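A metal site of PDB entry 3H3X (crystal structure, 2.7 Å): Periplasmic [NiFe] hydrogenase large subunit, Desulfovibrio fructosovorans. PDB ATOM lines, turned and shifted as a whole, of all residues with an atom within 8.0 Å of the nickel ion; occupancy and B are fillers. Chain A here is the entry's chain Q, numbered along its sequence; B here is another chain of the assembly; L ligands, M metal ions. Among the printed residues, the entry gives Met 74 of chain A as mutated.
SG of Cys 75 binds FE1 of the ligand.
The backbone NH of Ser 499 is in hydrogen-bond range of a nitrogen (N1) of the ligand (3.1 Å).
The side-chain sulfur (SG) of Cys 546 binds an iron atom (FE1) of the ligand, 2.4 Å away.
A nitrogen (N2) of the ligand lies within hydrogen-bond range of the backbone NH (N) of Arg 476 (2.8 Å).
OG of Ser 499 lies within hydrogen-bond range of N1 of the ligand (2.7 Å).
The guanidinium group (NH1) of Arg 476 sits close to a nitrogen (N2) of the ligand (3.5 Å).
The side-chain sulfur of Cys 546 sits close to a ring nitrogen (NE2) of His 79 (3.2 Å).
SG of Cys 543 sits close to OE1 of Glu 25, at 3.2 Å.
N of Cys 543 sits at hydrogen-bond distance from OG of Ser 499 (3.1 Å).
SG of Cys 72 lies close to N of Met 74 (3.4 Å).
Of the 29 residues printed, 4 come within 4 Å of the nickel ion.
The nearest printed residue that does not touch the nickel ion is Met 74 (4.6 Å).
The nickel ion is bound by SG of Cys 72 (2.1 Å), SG of Cys 543 (2.3 Å), SG of Cys 75 (2.4 Å) and SG of Cys 546 (2.5 Å).
The nickel ion has four donor atoms within binding distance.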
ATOM      1  N   GLU A  25       5.578  -7.686  21.925  1.00  0.00           N
ATOM      2  CA  GLU A  25       6.456  -7.324  20.830  1.00  0.00           C
ATOM      3  C   GLU A  25       5.620  -6.750  19.660  1.00  0.00           C
ATOM      4  O   GLU A  25       4.673  -7.407  19.164  1.00  0.00           O
ATOM      5  CB  GLU A  25       7.232  -8.557  20.365  1.00  0.00           C
ATOM      6  CG  GLU A  25       8.348  -8.251  19.375  1.00  0.00           C
ATOM      7  CD  GLU A  25       7.825  -7.628  18.131  1.00  0.00           C
ATOM      8  OE1 GLU A  25       6.755  -8.088  17.632  1.00  0.00           O
ATOM      9  OE2 GLU A  25       8.422  -6.611  17.659  1.00  0.00           O
ATOM     10  N   GLY A  26       5.958  -5.540  19.216  1.00  0.00           N
ATOM     11  CA  GLY A  26       5.405  -4.993  17.984  1.00  0.00           C
ATOM     12  C   GLY A  26       4.164  -4.112  18.159  1.00  0.00           C
ATOM     13  O   GLY A  26       3.872  -3.652  19.279  1.00  0.00           O
ATOM     14  N   ARG A  50       6.573  -5.047   7.228  1.00  0.00           N
ATOM     15  CA  ARG A  50       7.997  -4.951   6.841  1.00  0.00           C
ATOM     16  C   ARG A  50       8.288  -5.647   5.551  1.00  0.00           C
ATOM     17  O   ARG A  50       8.976  -5.087   4.740  1.00  0.00           O
ATOM     18  CB  ARG A  50       8.935  -5.448   7.946  1.00  0.00           C
ATOM     19  CG  ARG A  50       9.174  -4.447   9.028  1.00  0.00           C
ATOM     20  CD  ARG A  50       9.988  -5.064  10.138  1.00  0.00           C
ATOM     21  NE  ARG A  50       9.353  -6.254  10.684  1.00  0.00           N
ATOM     22  CZ  ARG A  50       9.993  -7.228  11.325  1.00  0.00           C
ATOM     23  NH1 ARG A  50      11.307  -7.154  11.496  1.00  0.00           N
ATOM     24  NH2 ARG A  50       9.347  -8.301  11.794  1.00  0.00           N
ATOM     25  N   GLN A  69      15.563 -14.526  10.801  1.00  0.00           N
ATOM     26  CA  GLN A  69      15.789 -14.330  12.255  1.00  0.00           C
ATOM     27  C   GLN A  69      15.308 -12.954  12.699  1.00  0.00           C
ATOM     28  O   GLN A  69      14.752 -12.813  13.779  1.00  0.00           O
ATOM     29  CB  GLN A  69      17.232 -14.585  12.702  1.00  0.00           C
ATOM     30  CG  GLN A  69      17.296 -14.549  14.230  1.00  0.00           C
ATOM     31  CD  GLN A  69      18.475 -15.273  14.889  1.00  0.00           C
ATOM     32  OE1 GLN A  69      18.372 -15.710  16.034  1.00  0.00           O
ATOM     33  NE2 GLN A  69      19.593 -15.392  14.186  1.00  0.00           N
ATOM     34  N   ALA A  71      12.858 -11.322  11.743  1.00  0.00           N
ATOM     35  CA  ALA A  71      11.419 -11.197  11.914  1.00  0.00           C
ATOM     36  C   ALA A  71      11.059 -10.814  13.325  1.00  0.00           C
ATOM     37  O   ALA A  71      10.057 -10.118  13.529  1.00  0.00           O
ATOM     38  CB  ALA A  71      10.681 -12.488  11.525  1.00  0.00           C
ATOM     39  N   CYS A  72      11.842 -11.259  14.290  1.00  0.00           N
ATOM     40  CA  CYS A  72      11.556 -11.007  15.688  1.00  0.00           C
ATOM     41  C   CYS A  72      12.803 -11.220  16.575  1.00  0.00           C
ATOM     42  O   CYS A  72      13.536 -12.226  16.465  1.00  0.00           O
ATOM     43  CB  CYS A  72      10.390 -11.881  16.217  1.00  0.00           C
ATOM     44  SG  CYS A  72       9.805 -11.328  17.886  1.00  0.00           S
ATOM     45  N   GLY A  73      13.021 -10.259  17.459  1.00  0.00           N
ATOM     46  CA  GLY A  73      14.143 -10.316  18.338  1.00  0.00           C
ATOM     47  C   GLY A  73      13.736 -10.734  19.732  1.00  0.00           C
ATOM     48  O   GLY A  73      14.605 -10.930  20.586  1.00  0.00           O
ATOM     49  N   MET A  74      12.424 -10.909  19.965  1.00  0.00           N
ATOM     50  CA  MET A  74      11.979 -11.416  21.254  1.00  0.00           C
ATOM     51  C   MET A  74      12.074 -12.948  21.201  1.00  0.00           C
ATOM     52  O   MET A  74      12.822 -13.570  22.012  1.00  0.00           O
ATOM     53  CB  MET A  74      10.598 -10.895  21.626  1.00  0.00           C
ATOM     54  CG  MET A  74      10.214 -11.267  23.000  1.00  0.00           C
ATOM     55  SD  MET A  74       8.681 -10.504  23.447  1.00  0.00           S
ATOM     56  CE  MET A  74       9.194  -8.802  23.732  1.00  0.00           C
ATOM     57  N   CYS A  75      11.350 -13.526  20.231  1.00  0.00           N
ATOM     58  CA  CYS A  75      11.460 -14.949  19.933  1.00  0.00           C
ATOM     59  C   CYS A  75      12.671 -15.124  18.981  1.00  0.00           C
ATOM     60  O   CYS A  75      12.578 -15.730  17.881  1.00  0.00           O
ATOM     61  CB  CYS A  75      10.160 -15.477  19.347  1.00  0.00           C
ATOM     62  SG  CYS A  75       9.813 -14.964  17.644  1.00  0.00           S
ATOM     63  N   THR A  76      13.799 -14.546  19.395  1.00  0.00           N
ATOM     64  CA  THR A  76      15.028 -14.691  18.618  1.00  0.00           C
ATOM     65  C   THR A  76      15.308 -16.192  18.416  1.00  0.00           C
ATOM     66  O   THR A  76      14.733 -17.040  19.118  1.00  0.00           O
ATOM     67  CB  THR A  76      16.232 -14.002  19.315  1.00  0.00           C
ATOM     68  OG1 THR A  76      17.346 -13.938  18.410  1.00  0.00           O
ATOM     69  CG2 THR A  76      16.656 -14.766  20.570  1.00  0.00           C
ATOM     70  N   VAL A  78      14.299 -18.678  16.912  1.00  0.00           N
ATOM     71  CA  VAL A  78      13.291 -19.612  16.349  1.00  0.00           C
ATOM     72  C   VAL A  78      13.135 -19.542  14.842  1.00  0.00           C
ATOM     73  O   VAL A  78      12.932 -20.584  14.214  1.00  0.00           O
ATOM     74  CB  VAL A  78      11.903 -19.569  17.061  1.00  0.00           C
ATOM     75  CG1 VAL A  78      12.081 -19.848  18.601  1.00  0.00           C
ATOM     76  CG2 VAL A  78      11.110 -18.240  16.781  1.00  0.00           C
ATOM     77  N   HIS A  79      13.278 -18.350  14.251  1.00  0.00           N
ATOM     78  CA  HIS A  79      13.114 -18.212  12.806  1.00  0.00           C
ATOM     79  C   HIS A  79      14.356 -18.670  12.058  1.00  0.00           C
ATOM     80  O   HIS A  79      14.269 -19.190  10.931  1.00  0.00           O
ATOM     81  CB  HIS A  79      12.773 -16.776  12.435  1.00  0.00           C
ATOM     82  CG  HIS A  79      11.393 -16.364  12.785  1.00  0.00           C
ATOM     83  ND1 HIS A  79      10.288 -16.690  12.019  1.00  0.00           N
ATOM     84  CD2 HIS A  79      10.929 -15.582  13.790  1.00  0.00           C
ATOM     85  CE1 HIS A  79       9.208 -16.155  12.549  1.00  0.00           C
ATOM     86  NE2 HIS A  79       9.565 -15.481  13.626  1.00  0.00           N
ATOM     87  N   GLN A 110      15.695 -20.888  24.916  1.00  0.00           N
ATOM     88  CA  GLN A 110      14.772 -19.858  24.480  1.00  0.00           C
ATOM     89  C   GLN A 110      13.444 -19.930  25.214  1.00  0.00           C
ATOM     90  O   GLN A 110      12.928 -18.878  25.638  1.00  0.00           O
ATOM     91  CB  GLN A 110      14.564 -19.873  22.952  1.00  0.00           C
ATOM     92  CG  GLN A 110      13.664 -18.794  22.356  1.00  0.00           C
ATOM     93  CD  GLN A 110      14.060 -17.360  22.727  1.00  0.00           C
ATOM     94  OE1 GLN A 110      15.250 -17.008  22.818  1.00  0.00           O
ATOM     95  NE2 GLN A 110      13.037 -16.512  22.957  1.00  0.00           N
ATOM     96  N   ASP A 114      12.192 -16.779  27.397  1.00  0.00           N
ATOM     97  CA  ASP A 114      11.021 -16.084  26.864  1.00  0.00           C
ATOM     98  C   ASP A 114       9.856 -16.073  27.864  1.00  0.00           C
ATOM     99  O   ASP A 114       9.269 -15.019  28.181  1.00  0.00           O
ATOM    100  CB  ASP A 114      10.559 -16.771  25.584  1.00  0.00           C
ATOM    101  CG  ASP A 114       9.927 -15.800  24.566  1.00  0.00           C
ATOM    102  OD1 ASP A 114       9.186 -14.877  24.989  1.00  0.00           O
ATOM    103  OD2 ASP A 114      10.161 -15.979  23.344  1.00  0.00           O
ATOM    104  N   ALA A 474       7.698 -22.886  18.392  1.00  0.00           N
ATOM    105  CA  ALA A 474       8.359 -21.776  19.031  1.00  0.00           C
ATOM    106  C   ALA A 474       7.667 -21.527  20.362  1.00  0.00           C
ATOM    107  O   ALA A 474       6.638 -22.125  20.641  1.00  0.00           O
ATOM    108  CB  ALA A 474       8.290 -20.556  18.113  1.00  0.00           C
ATOM    109  N   PRO A 475       8.248 -20.650  21.216  1.00  0.00           N
ATOM    110  CA  PRO A 475       7.549 -20.319  22.479  1.00  0.00           C
ATOM    111  C   PRO A 475       6.079 -19.907  22.330  1.00  0.00           C
ATOM    112  O   PRO A 475       5.260 -20.190  23.209  1.00  0.00           O
ATOM    113  CB  PRO A 475       8.391 -19.156  23.032  1.00  0.00           C
ATOM    114  CG  PRO A 475       9.800 -19.511  22.558  1.00  0.00           C
ATOM    115  CD  PRO A 475       9.565 -19.977  21.122  1.00  0.00           C
ATOM    116  N   ARG A 476       5.722 -19.275  21.232  1.00  0.00           N
ATOM    117  CA  ARG A 476       4.358 -18.813  21.072  1.00  0.00           C
ATOM    118  C   ARG A 476       3.431 -19.767  20.326  1.00  0.00           C
ATOM    119  O   ARG A 476       2.213 -19.560  20.310  1.00  0.00           O
ATOM    120  CB  ARG A 476       4.356 -17.423  20.454  1.00  0.00           C
ATOM    121  CG  ARG A 476       4.607 -16.381  21.487  1.00  0.00           C
ATOM    122  CD  ARG A 476       5.176 -15.141  20.942  1.00  0.00           C
ATOM    123  NE  ARG A 476       5.645 -14.299  22.066  1.00  0.00           N
ATOM    124  CZ  ARG A 476       6.857 -14.365  22.615  1.00  0.00           C
ATOM    125  NH1 ARG A 476       7.777 -15.192  22.164  1.00  0.00           N
ATOM    126  NH2 ARG A 476       7.179 -13.574  23.613  1.00  0.00           N
ATOM    127  N   VAL A 497       3.399 -17.912  11.039  1.00  0.00           N
ATOM    128  CA  VAL A 497       3.986 -17.731  12.331  1.00  0.00           C
ATOM    129  C   VAL A 497       2.925 -17.857  13.428  1.00  0.00           C
ATOM    130  O   VAL A 497       1.749 -17.530  13.155  1.00  0.00           O
ATOM    131  CB  VAL A 497       4.700 -16.376  12.405  1.00  0.00           C
ATOM    132  CG1 VAL A 497       5.601 -16.289  13.597  1.00  0.00           C
ATOM    133  CG2 VAL A 497       5.570 -16.228  11.225  1.00  0.00           C
ATOM    134  N   PRO A 498       3.307 -18.382  14.645  1.00  0.00           N
ATOM    135  CA  PRO A 498       2.306 -18.556  15.691  1.00  0.00           C
ATOM    136  C   PRO A 498       1.390 -17.349  15.856  1.00  0.00           C
ATOM    137  O   PRO A 498       0.188 -17.544  15.841  1.00  0.00           O
ATOM    138  CB  PRO A 498       3.155 -18.777  16.978  1.00  0.00           C
ATOM    139  CG  PRO A 498       4.577 -18.778  16.564  1.00  0.00           C
ATOM    140  CD  PRO A 498       4.636 -18.860  15.089  1.00  0.00           C
ATOM    141  N   SER A 499       1.932 -16.127  15.981  1.00  0.00           N
ATOM    142  CA  SER A 499       1.083 -14.951  16.178  1.00  0.00           C
ATOM    143  C   SER A 499       0.158 -14.699  14.993  1.00  0.00           C
ATOM    144  O   SER A 499      -0.953 -14.206  15.181  1.00  0.00           O
ATOM    145  CB  SER A 499       1.888 -13.699  16.494  1.00  0.00           C
ATOM    146  OG  SER A 499       2.369 -13.757  17.839  1.00  0.00           O
ATOM    147  N   ASP A 541       0.460 -13.928  24.446  1.00  0.00           N
ATOM    148  CA  ASP A 541       1.853 -13.540  24.303  1.00  0.00           C
ATOM    149  C   ASP A 541       2.151 -13.017  22.875  1.00  0.00           C
ATOM    150  O   ASP A 541       3.012 -13.570  22.196  1.00  0.00           O
ATOM    151  CB  ASP A 541       2.751 -14.745  24.729  1.00  0.00           C
ATOM    152  CG  ASP A 541       4.253 -14.450  24.607  1.00  0.00           C
ATOM    153  OD1 ASP A 541       4.651 -13.255  24.498  1.00  0.00           O
ATOM    154  OD2 ASP A 541       5.055 -15.445  24.578  1.00  0.00           O
ATOM    155  N   PRO A 542       1.465 -11.941  22.441  1.00  0.00           N
ATOM    156  CA  PRO A 542       1.495 -11.453  21.050  1.00  0.00           C
ATOM    157  C   PRO A 542       2.838 -10.891  20.613  1.00  0.00           C
ATOM    158  O   PRO A 542       3.521 -10.190  21.396  1.00  0.00           O
ATOM    159  CB  PRO A 542       0.464 -10.309  21.028  1.00  0.00           C
ATOM    160  CG  PRO A 542      -0.295 -10.432  22.252  1.00  0.00           C
ATOM    161  CD  PRO A 542       0.612 -11.066  23.265  1.00  0.00           C
ATOM    162  N   CYS A 543       3.172 -11.169  19.361  1.00  0.00           N
ATOM    163  CA  CYS A 543       4.393 -10.711  18.719  1.00  0.00           C
ATOM    164  C   CYS A 543       4.016 -10.335  17.283  1.00  0.00           C
ATOM    165  O   CYS A 543       3.826 -11.200  16.406  1.00  0.00           O
ATOM    166  CB  CYS A 543       5.472 -11.810  18.757  1.00  0.00           C
ATOM    167  SG  CYS A 543       7.072 -11.249  18.135  1.00  0.00           S
ATOM    168  N   ILE A 544       3.902  -9.028  17.061  1.00  0.00           N
ATOM    169  CA  ILE A 544       3.333  -8.495  15.823  1.00  0.00           C
ATOM    170  C   ILE A 544       4.397  -8.480  14.740  1.00  0.00           C
ATOM    171  O   ILE A 544       4.115  -8.734  13.534  1.00  0.00           O
ATOM    172  CB  ILE A 544       2.721  -7.086  16.039  1.00  0.00           C
ATOM    173  CG1 ILE A 544       1.775  -7.048  17.255  1.00  0.00           C
ATOM    174  CG2 ILE A 544       2.006  -6.585  14.765  1.00  0.00           C
ATOM    175  CD1 ILE A 544       0.706  -8.150  17.365  1.00  0.00           C
ATOM    176  N   ALA A 545       5.637  -8.247  15.126  1.00  0.00           N
ATOM    177  CA  ALA A 545       6.715  -8.373  14.138  1.00  0.00           C
ATOM    178  C   ALA A 545       6.791  -9.817  13.618  1.00  0.00           C
ATOM    179  O   ALA A 545       6.900 -10.040  12.442  1.00  0.00           O
ATOM    180  CB  ALA A 545       8.011  -7.909  14.746  1.00  0.00           C
ATOM    181  N   CYS A 546       6.689 -10.785  14.530  1.00  0.00           N
ATOM    182  CA  CYS A 546       6.511 -12.196  14.132  1.00  0.00           C
ATOM    183  C   CYS A 546       5.346 -12.423  13.174  1.00  0.00           C
ATOM    184  O   CYS A 546       5.522 -13.053  12.132  1.00  0.00           O
ATOM    185  CB  CYS A 546       6.315 -13.098  15.361  1.00  0.00           C
ATOM    186  SG  CYS A 546       7.757 -13.922  15.813  1.00  0.00           S
ATOM    187  N   GLY A 547       4.160 -11.935  13.554  1.00  0.00           N
ATOM    188  CA  GLY A 547       2.908 -12.219  12.850  1.00  0.00           C
ATOM    189  C   GLY A 547       2.846 -11.656  11.439  1.00  0.00           C
ATOM    190  O   GLY A 547       2.333 -12.321  10.554  1.00  0.00           O
ATOM    191  N   CYS B  17      12.297  -5.236  15.419  1.00  0.00           N
ATOM    192  CA  CYS B  17      11.976  -6.582  15.774  1.00  0.00           C
ATOM    193  C   CYS B  17      12.068  -6.711  17.259  1.00  0.00           C
ATOM    194  O   CYS B  17      11.841  -7.786  17.768  1.00  0.00           O
ATOM    195  CB  CYS B  17      12.971  -7.546  15.104  1.00  0.00           C
ATOM    196  SG  CYS B  17      14.616  -7.607  15.918  1.00  0.00           S
ATOM    197  N   THR B  18      12.411  -5.624  17.940  1.00  0.00           N
ATOM    198  CA  THR B  18      12.532  -5.557  19.423  1.00  0.00           C
ATOM    199  C   THR B  18      13.802  -6.254  19.998  1.00  0.00           C
ATOM    200  O   THR B  18      14.006  -6.304  21.203  1.00  0.00           O
ATOM    201  CB  THR B  18      11.193  -5.997  20.125  1.00  0.00           C
ATOM    202  OG1 THR B  18      10.073  -5.386  19.429  1.00  0.00           O
ATOM    203  CG2 THR B  18      11.135  -5.586  21.600  1.00  0.00           C
HETATM  204 FE1  LIG L   1       7.659 -15.530  17.531  1.00  0.00          FE
HETATM  205  C1  LIG L   1       5.742 -15.398  17.317  1.00  0.00           C
HETATM  206  N1  LIG L   1       4.590 -15.218  17.238  1.00  0.00           N
HETATM  207  C2  LIG L   1       7.607 -16.863  18.917  1.00  0.00           C
HETATM  208  N2  LIG L   1       7.567 -17.670  19.770  1.00  0.00           N
HETATM  209  C3  LIG L   1       7.646 -16.818  16.423  1.00  0.00           C
HETATM  210  O1  LIG L   1       7.676 -17.632  15.676  1.00  0.00           O
HETATM  211 NI    NI M   1       8.515 -12.979  18.040  1.00  0.00          NI
